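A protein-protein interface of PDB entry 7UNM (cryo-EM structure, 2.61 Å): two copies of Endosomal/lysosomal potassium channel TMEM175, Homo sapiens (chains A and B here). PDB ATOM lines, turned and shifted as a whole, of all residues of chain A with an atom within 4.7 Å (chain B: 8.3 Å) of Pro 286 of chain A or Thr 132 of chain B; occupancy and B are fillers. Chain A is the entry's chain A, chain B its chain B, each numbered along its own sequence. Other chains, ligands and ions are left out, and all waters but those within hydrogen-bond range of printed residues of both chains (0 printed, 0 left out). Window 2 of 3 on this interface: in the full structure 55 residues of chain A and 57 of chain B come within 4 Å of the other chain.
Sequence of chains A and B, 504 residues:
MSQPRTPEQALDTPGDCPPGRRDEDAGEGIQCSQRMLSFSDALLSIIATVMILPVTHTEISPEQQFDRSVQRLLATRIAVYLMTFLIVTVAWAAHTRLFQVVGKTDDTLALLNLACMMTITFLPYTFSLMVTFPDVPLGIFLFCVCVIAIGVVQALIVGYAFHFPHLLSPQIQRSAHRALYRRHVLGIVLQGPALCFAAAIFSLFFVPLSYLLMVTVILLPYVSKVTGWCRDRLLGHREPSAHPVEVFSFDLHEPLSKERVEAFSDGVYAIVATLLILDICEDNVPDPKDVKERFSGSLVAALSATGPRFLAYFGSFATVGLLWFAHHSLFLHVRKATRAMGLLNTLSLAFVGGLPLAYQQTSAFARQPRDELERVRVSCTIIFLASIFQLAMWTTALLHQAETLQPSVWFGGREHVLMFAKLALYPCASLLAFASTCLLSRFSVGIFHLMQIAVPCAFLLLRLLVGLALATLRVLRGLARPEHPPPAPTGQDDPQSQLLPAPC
The backbone carbonyl oxygen (O) of Ser 128 of chain B lies within hydrogen-bond range of the side-chain hydroxyl (OG1) of Thr 132 of chain B (3.3 Å). The side-chain hydroxyl (OG1) of Thr 132 of chain B lies within hydrogen-bond range of the backbone carbonyl oxygen (O) of Leu 129 of chain B, at 2.5 Å.
The side-chain hydroxyl (OH) of Tyr 125 of chain B lies within hydrogen-bond range of the backbone carbonyl oxygen (O) of Asn 284 of chain A (3.1 Å).
No position is printed for both chains.
Printed residues of chain B that touch a printed residue of chain A: Tyr 125, Ser 128, Leu 129, Thr 132 and Phe 133. Along chain B the printed residues that touch a printed residue of chain A span positions 125 to 133. Of the 8 printed residues of chain A, 5 touch a printed residue of chain B. Along chain A the printed residues that touch a printed residue of chain B span positions 284 to 288. Among the printed residues, 7 pairs touch across the chains. Among the printed residues, no Asp or Glu carboxylate lies within 4 Å of a Lys or Arg side-chain nitrogen of the other chain.
CD1 of Leu 129 of chain B touches O of Asn 284 of chain A, at 3.9 Å. CG1 of Val 285 of chain A touches OG of Ser 128 of chain B, 3.5 Å away. Pro 286 of chain A touches Thr 132 of chain B. Pro 286 of chain A touches Phe 133 of chain B. Asp 287 of chain A touches Phe 133 of chain B (C to CZ, 3.4 Å). Phe 133 of chain B touches Pro 288 of chain A (CE1 to N, 3.3 Å).
Thr 132 of chain B touches just one residue of chain A: Pro 286 (3.6 Å). Printed residues of chain B within 4 Å of Asp 287 of chain A: Phe 133 (3.4 Å). Of the printed residues of chain A, Phe 133 of chain B touches Pro 286, Asp 287 and Pro 288. Thr 126 of chain B touches none of the printed residues of chain A. Pro 134 of chain B touches none of the printed residues of chain A. The nearest residue of chain A that does not touch Thr 132 of chain B is Val 285 of chain A (4.3 Å).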
ATOM      1  N   ASN A 284     -19.801 -11.448  23.426  1.00  0.00           N
ATOM      2  CA  ASN A 284     -18.866 -12.325  24.125  1.00  0.00           C
ATOM      3  C   ASN A 284     -18.071 -11.557  25.173  1.00  0.00           C
ATOM      4  O   ASN A 284     -16.842 -11.624  25.231  1.00  0.00           O
ATOM      5  CB  ASN A 284     -17.939 -13.002  23.121  1.00  0.00           C
ATOM      6  CG  ASN A 284     -18.697 -13.788  22.072  1.00  0.00           C
ATOM      7  OD1 ASN A 284     -18.673 -13.452  20.889  1.00  0.00           O
ATOM      8  ND2 ASN A 284     -19.384 -14.839  22.503  1.00  0.00           N
ATOM      9  N   VAL A 285     -18.772 -10.811  26.021  1.00  0.00           N
ATOM     10  CA  VAL A 285     -18.139 -10.089  27.123  1.00  0.00           C
ATOM     11  C   VAL A 285     -18.841 -10.464  28.423  1.00  0.00           C
ATOM     12  O   VAL A 285     -19.652  -9.682  28.941  1.00  0.00           O
ATOM     13  CB  VAL A 285     -18.168  -8.570  26.880  1.00  0.00           C
ATOM     14  CG1 VAL A 285     -17.150  -8.194  25.819  1.00  0.00           C
ATOM     15  CG2 VAL A 285     -19.562  -8.114  26.457  1.00  0.00           C
ATOM     16  N   PRO A 286     -18.554 -11.633  28.993  1.00  0.00           N
ATOM     17  CA  PRO A 286     -19.279 -12.069  30.191  1.00  0.00           C
ATOM     18  C   PRO A 286     -18.976 -11.192  31.395  1.00  0.00           C
ATOM     19  O   PRO A 286     -18.023 -10.409  31.415  1.00  0.00           O
ATOM     20  CB  PRO A 286     -18.779 -13.502  30.413  1.00  0.00           C
ATOM     21  CG  PRO A 286     -18.131 -13.906  29.126  1.00  0.00           C
ATOM     22  CD  PRO A 286     -17.591 -12.646  28.536  1.00  0.00           C
ATOM     23  N   ASP A 287     -19.821 -11.334  32.410  1.00  0.00           N
ATOM     24  CA  ASP A 287     -19.672 -10.664  33.691  1.00  0.00           C
ATOM     25  C   ASP A 287     -19.255 -11.658  34.767  1.00  0.00           C
ATOM     26  O   ASP A 287     -19.438 -12.870  34.612  1.00  0.00           O
ATOM     27  CB  ASP A 287     -20.984  -9.983  34.107  1.00  0.00           C
ATOM     28  CG  ASP A 287     -21.249  -8.707  33.334  1.00  0.00           C
ATOM     29  OD1 ASP A 287     -20.403  -8.331  32.496  1.00  0.00           O
ATOM     30  OD2 ASP A 287     -22.303  -8.079  33.565  1.00  0.00           O
ATOM     31  N   PRO A 288     -18.679 -11.181  35.876  1.00  0.00           N
ATOM     32  CA  PRO A 288     -18.234 -12.124  36.918  1.00  0.00           C
ATOM     33  C   PRO A 288     -19.337 -13.045  37.408  1.00  0.00           C
ATOM     34  O   PRO A 288     -19.092 -14.240  37.619  1.00  0.00           O
ATOM     35  CB  PRO A 288     -17.728 -11.195  38.032  1.00  0.00           C
ATOM     36  CG  PRO A 288     -17.388  -9.919  37.344  1.00  0.00           C
ATOM     37  CD  PRO A 288     -18.377  -9.783  36.227  1.00  0.00           C
ATOM     38  N   ASP A 290     -21.660 -14.214  35.731  1.00  0.00           N
ATOM     39  CA  ASP A 290     -21.924 -15.193  34.686  1.00  0.00           C
ATOM     40  C   ASP A 290     -20.788 -16.198  34.546  1.00  0.00           C
ATOM     41  O   ASP A 290     -21.039 -17.392  34.349  1.00  0.00           O
ATOM     42  CB  ASP A 290     -22.156 -14.484  33.349  1.00  0.00           C
ATOM     43  CG  ASP A 290     -22.492 -15.449  32.229  1.00  0.00           C
ATOM     44  OD1 ASP A 290     -22.907 -16.588  32.527  1.00  0.00           O
ATOM     45  OD2 ASP A 290     -22.339 -15.068  31.048  1.00  0.00           O
ATOM     46  N   ARG A 294     -21.398 -20.225  34.881  1.00  0.00           N
ATOM     47  CA  ARG A 294     -21.378 -21.068  33.690  1.00  0.00           C
ATOM     48  C   ARG A 294     -20.080 -21.856  33.570  1.00  0.00           C
ATOM     49  O   ARG A 294     -20.087 -22.976  33.047  1.00  0.00           O
ATOM     50  CB  ARG A 294     -21.592 -20.215  32.439  1.00  0.00           C
ATOM     51  CG  ARG A 294     -23.046 -19.848  32.181  1.00  0.00           C
ATOM     52  CD  ARG A 294     -23.280 -19.475  30.724  1.00  0.00           C
ATOM     53  NE  ARG A 294     -22.638 -18.216  30.370  1.00  0.00           N
ATOM     54  CZ  ARG A 294     -22.331 -17.849  29.133  1.00  0.00           C
ATOM     55  NH1 ARG A 294     -22.597 -18.624  28.093  1.00  0.00           N
ATOM     56  NH2 ARG A 294     -21.743 -16.673  28.932  1.00  0.00           N
ATOM     57  N   THR A 306     -17.000 -18.694  23.681  1.00  0.00           N
ATOM     58  CA  THR A 306     -16.677 -17.414  23.061  1.00  0.00           C
ATOM     59  C   THR A 306     -15.584 -17.512  22.006  1.00  0.00           C
ATOM     60  O   THR A 306     -15.500 -16.634  21.142  1.00  0.00           O
ATOM     61  CB  THR A 306     -16.243 -16.397  24.125  1.00  0.00           C
ATOM     62  OG1 THR A 306     -15.040 -16.842  24.762  1.00  0.00           O
ATOM     63  CG2 THR A 306     -17.331 -16.221  25.175  1.00  0.00           C
ATOM     64  N   VAL B  80     -11.810   4.569  30.379  1.00  0.00           N
ATOM     65  CA  VAL B  80     -11.634   3.486  29.416  1.00  0.00           C
ATOM     66  C   VAL B  80     -11.888   3.992  28.004  1.00  0.00           C
ATOM     67  O   VAL B  80     -11.151   3.663  27.068  1.00  0.00           O
ATOM     68  CB  VAL B  80     -12.558   2.305  29.769  1.00  0.00           C
ATOM     69  CG1 VAL B  80     -12.753   1.393  28.565  1.00  0.00           C
ATOM     70  CG2 VAL B  80     -11.997   1.529  30.946  1.00  0.00           C
ATOM     71  N   TYR B 125     -12.735  -5.078  21.218  1.00  0.00           N
ATOM     72  CA  TYR B 125     -13.237  -6.283  21.870  1.00  0.00           C
ATOM     73  C   TYR B 125     -12.287  -6.749  22.965  1.00  0.00           C
ATOM     74  O   TYR B 125     -12.716  -7.083  24.077  1.00  0.00           O
ATOM     75  CB  TYR B 125     -13.449  -7.387  20.834  1.00  0.00           C
ATOM     76  CG  TYR B 125     -13.788  -8.729  21.438  1.00  0.00           C
ATOM     77  CD1 TYR B 125     -15.016  -8.950  22.046  1.00  0.00           C
ATOM     78  CD2 TYR B 125     -12.878  -9.775  21.403  1.00  0.00           C
ATOM     79  CE1 TYR B 125     -15.328 -10.174  22.599  1.00  0.00           C
ATOM     80  CE2 TYR B 125     -13.182 -11.003  21.955  1.00  0.00           C
ATOM     81  CZ  TYR B 125     -14.407 -11.198  22.550  1.00  0.00           C
ATOM     82  OH  TYR B 125     -14.713 -12.422  23.102  1.00  0.00           O
ATOM     83  N   THR B 126     -10.985  -6.770  22.672  1.00  0.00           N
ATOM     84  CA  THR B 126     -10.012  -7.190  23.675  1.00  0.00           C
ATOM     85  C   THR B 126      -9.991  -6.227  24.852  1.00  0.00           C
ATOM     86  O   THR B 126      -9.910  -6.653  26.012  1.00  0.00           O
ATOM     87  CB  THR B 126      -8.621  -7.295  23.049  1.00  0.00           C
ATOM     88  OG1 THR B 126      -8.259  -6.035  22.471  1.00  0.00           O
ATOM     89  CG2 THR B 126      -8.600  -8.367  21.974  1.00  0.00           C
ATOM     90  N   PHE B 127     -10.058  -4.923  24.578  1.00  0.00           N
ATOM     91  CA  PHE B 127     -10.039  -3.954  25.669  1.00  0.00           C
ATOM     92  C   PHE B 127     -11.283  -4.091  26.540  1.00  0.00           C
ATOM     93  O   PHE B 127     -11.198  -4.004  27.770  1.00  0.00           O
ATOM     94  CB  PHE B 127      -9.919  -2.535  25.115  1.00  0.00           C
ATOM     95  CG  PHE B 127      -9.218  -1.582  26.044  1.00  0.00           C
ATOM     96  CD1 PHE B 127      -7.834  -1.502  26.056  1.00  0.00           C
ATOM     97  CD2 PHE B 127      -9.936  -0.776  26.910  1.00  0.00           C
ATOM     98  CE1 PHE B 127      -7.182  -0.631  26.909  1.00  0.00           C
ATOM     99  CE2 PHE B 127      -9.289   0.099  27.765  1.00  0.00           C
ATOM    100  CZ  PHE B 127      -7.910   0.170  27.764  1.00  0.00           C
ATOM    101  N   SER B 128     -12.444  -4.319  25.923  1.00  0.00           N
ATOM    102  CA  SER B 128     -13.665  -4.534  26.692  1.00  0.00           C
ATOM    103  C   SER B 128     -13.569  -5.792  27.543  1.00  0.00           C
ATOM    104  O   SER B 128     -13.982  -5.797  28.708  1.00  0.00           O
ATOM    105  CB  SER B 128     -14.865  -4.623  25.750  1.00  0.00           C
ATOM    106  OG  SER B 128     -16.044  -4.962  26.461  1.00  0.00           O
ATOM    107  N   LEU B 129     -13.036  -6.876  26.975  1.00  0.00           N
ATOM    108  CA  LEU B 129     -12.899  -8.105  27.746  1.00  0.00           C
ATOM    109  C   LEU B 129     -11.963  -7.901  28.929  1.00  0.00           C
ATOM    110  O   LEU B 129     -12.219  -8.405  30.029  1.00  0.00           O
ATOM    111  CB  LEU B 129     -12.395  -9.237  26.853  1.00  0.00           C
ATOM    112  CG  LEU B 129     -12.446 -10.625  27.494  1.00  0.00           C
ATOM    113  CD1 LEU B 129     -13.885 -11.087  27.657  1.00  0.00           C
ATOM    114  CD2 LEU B 129     -11.646 -11.621  26.676  1.00  0.00           C
ATOM    115  N   MET B 130     -10.868  -7.168  28.721  1.00  0.00           N
ATOM    116  CA  MET B 130      -9.970  -6.861  29.827  1.00  0.00           C
ATOM    117  C   MET B 130     -10.670  -6.006  30.877  1.00  0.00           C
ATOM    118  O   MET B 130     -10.463  -6.192  32.081  1.00  0.00           O
ATOM    119  CB  MET B 130      -8.718  -6.160  29.300  1.00  0.00           C
ATOM    120  CG  MET B 130      -7.682  -5.841  30.364  1.00  0.00           C
ATOM    121  SD  MET B 130      -6.219  -5.043  29.675  1.00  0.00           S
ATOM    122  CE  MET B 130      -6.867  -3.422  29.281  1.00  0.00           C
ATOM    123  N   VAL B 131     -11.504  -5.061  30.436  1.00  0.00           N
ATOM    124  CA  VAL B 131     -12.231  -4.210  31.373  1.00  0.00           C
ATOM    125  C   VAL B 131     -13.176  -5.043  32.229  1.00  0.00           C
ATOM    126  O   VAL B 131     -13.284  -4.833  33.443  1.00  0.00           O
ATOM    127  CB  VAL B 131     -12.987  -3.105  30.611  1.00  0.00           C
ATOM    128  CG1 VAL B 131     -13.993  -2.419  31.524  1.00  0.00           C
ATOM    129  CG2 VAL B 131     -12.009  -2.091  30.043  1.00  0.00           C
ATOM    130  N   THR B 132     -13.882  -5.991  31.613  1.00  0.00           N
ATOM    131  CA  THR B 132     -14.828  -6.806  32.369  1.00  0.00           C
ATOM    132  C   THR B 132     -14.119  -7.626  33.440  1.00  0.00           C
ATOM    133  O   THR B 132     -14.606  -7.736  34.572  1.00  0.00           O
ATOM    134  CB  THR B 132     -15.608  -7.725  31.427  1.00  0.00           C
ATOM    135  OG1 THR B 132     -14.694  -8.441  30.587  1.00  0.00           O
ATOM    136  CG2 THR B 132     -16.562  -6.916  30.562  1.00  0.00           C
ATOM    137  N   PHE B 133     -12.966  -8.206  33.105  1.00  0.00           N
ATOM    138  CA  PHE B 133     -12.195  -9.044  34.023  1.00  0.00           C
ATOM    139  C   PHE B 133     -10.755  -8.550  34.027  1.00  0.00           C
ATOM    140  O   PHE B 133      -9.866  -9.180  33.438  1.00  0.00           O
ATOM    141  CB  PHE B 133     -12.272 -10.516  33.622  1.00  0.00           C
ATOM    142  CG  PHE B 133     -13.675 -11.029  33.484  1.00  0.00           C
ATOM    143  CD1 PHE B 133     -14.488 -11.164  34.593  1.00  0.00           C
ATOM    144  CD2 PHE B 133     -14.179 -11.375  32.243  1.00  0.00           C
ATOM    145  CE1 PHE B 133     -15.779 -11.634  34.469  1.00  0.00           C
ATOM    146  CE2 PHE B 133     -15.469 -11.846  32.112  1.00  0.00           C
ATOM    147  CZ  PHE B 133     -16.270 -11.976  33.227  1.00  0.00           C
ATOM    148  N   PRO B 134     -10.487  -7.418  34.684  1.00  0.00           N
ATOM    149  CA  PRO B 134      -9.120  -6.876  34.676  1.00  0.00           C
ATOM    150  C   PRO B 134      -8.109  -7.746  35.400  1.00  0.00           C
ATOM    151  O   PRO B 134      -6.906  -7.597  35.151  1.00  0.00           O
ATOM    152  CB  PRO B 134      -9.278  -5.515  35.367  1.00  0.00           C
ATOM    153  CG  PRO B 134     -10.467  -5.683  36.250  1.00  0.00           C
ATOM    154  CD  PRO B 134     -11.392  -6.627  35.535  1.00  0.00           C
ATOM    155  N   ASP B 135      -8.548  -8.644  36.279  1.00  0.00           N
ATOM    156  CA  ASP B 135      -7.645  -9.454  37.086  1.00  0.00           C
ATOM    157  C   ASP B 135      -7.349 -10.813  36.465  1.00  0.00           C
ATOM    158  O   ASP B 135      -6.626 -11.611  37.068  1.00  0.00           O
ATOM    159  CB  ASP B 135      -8.223  -9.641  38.491  1.00  0.00           C
ATOM    160  CG  ASP B 135      -9.575 -10.327  38.478  1.00  0.00           C
ATOM    161  OD1 ASP B 135     -10.143 -10.505  37.379  1.00  0.00           O
ATOM    162  OD2 ASP B 135     -10.071 -10.688  39.566  1.00  0.00           O
ATOM    163  N   VAL B 136      -7.882 -11.096  35.279  1.00  0.00           N
ATOM    164  CA  VAL B 136      -7.639 -12.374  34.614  1.00  0.00           C
ATOM    165  C   VAL B 136      -6.649 -12.147  33.475  1.00  0.00           C
ATOM    166  O   VAL B 136      -6.723 -11.114  32.794  1.00  0.00           O
ATOM    167  CB  VAL B 136      -8.945 -12.997  34.100  1.00  0.00           C
ATOM    168  CG1 VAL B 136      -8.681 -14.385  33.540  1.00  0.00           C
ATOM    169  CG2 VAL B 136      -9.981 -13.056  35.213  1.00  0.00           C
ATOM    170  N   LEU B 138      -6.562 -13.233  30.572  1.00  0.00           N
ATOM    171  CA  LEU B 138      -7.094 -13.391  29.221  1.00  0.00           C
ATOM    172  C   LEU B 138      -7.108 -12.067  28.465  1.00  0.00           C
ATOM    173  O   LEU B 138      -6.724 -12.005  27.291  1.00  0.00           O
ATOM    174  CB  LEU B 138      -8.501 -13.987  29.281  1.00  0.00           C
ATOM    175  CG  LEU B 138      -9.234 -14.091  27.941  1.00  0.00           C
ATOM    176  CD1 LEU B 138      -8.412 -14.879  26.932  1.00  0.00           C
ATOM    177  CD2 LEU B 138     -10.603 -14.727  28.129  1.00  0.00           C
ATOM    178  N   GLY B 139      -7.566 -10.996  29.117  1.00  0.00           N
ATOM    179  CA  GLY B 139      -7.669  -9.719  28.427  1.00  0.00           C
ATOM    180  C   GLY B 139      -6.318  -9.195  27.982  1.00  0.00           C
ATOM    181  O   GLY B 139      -6.147  -8.760  26.839  1.00  0.00           O
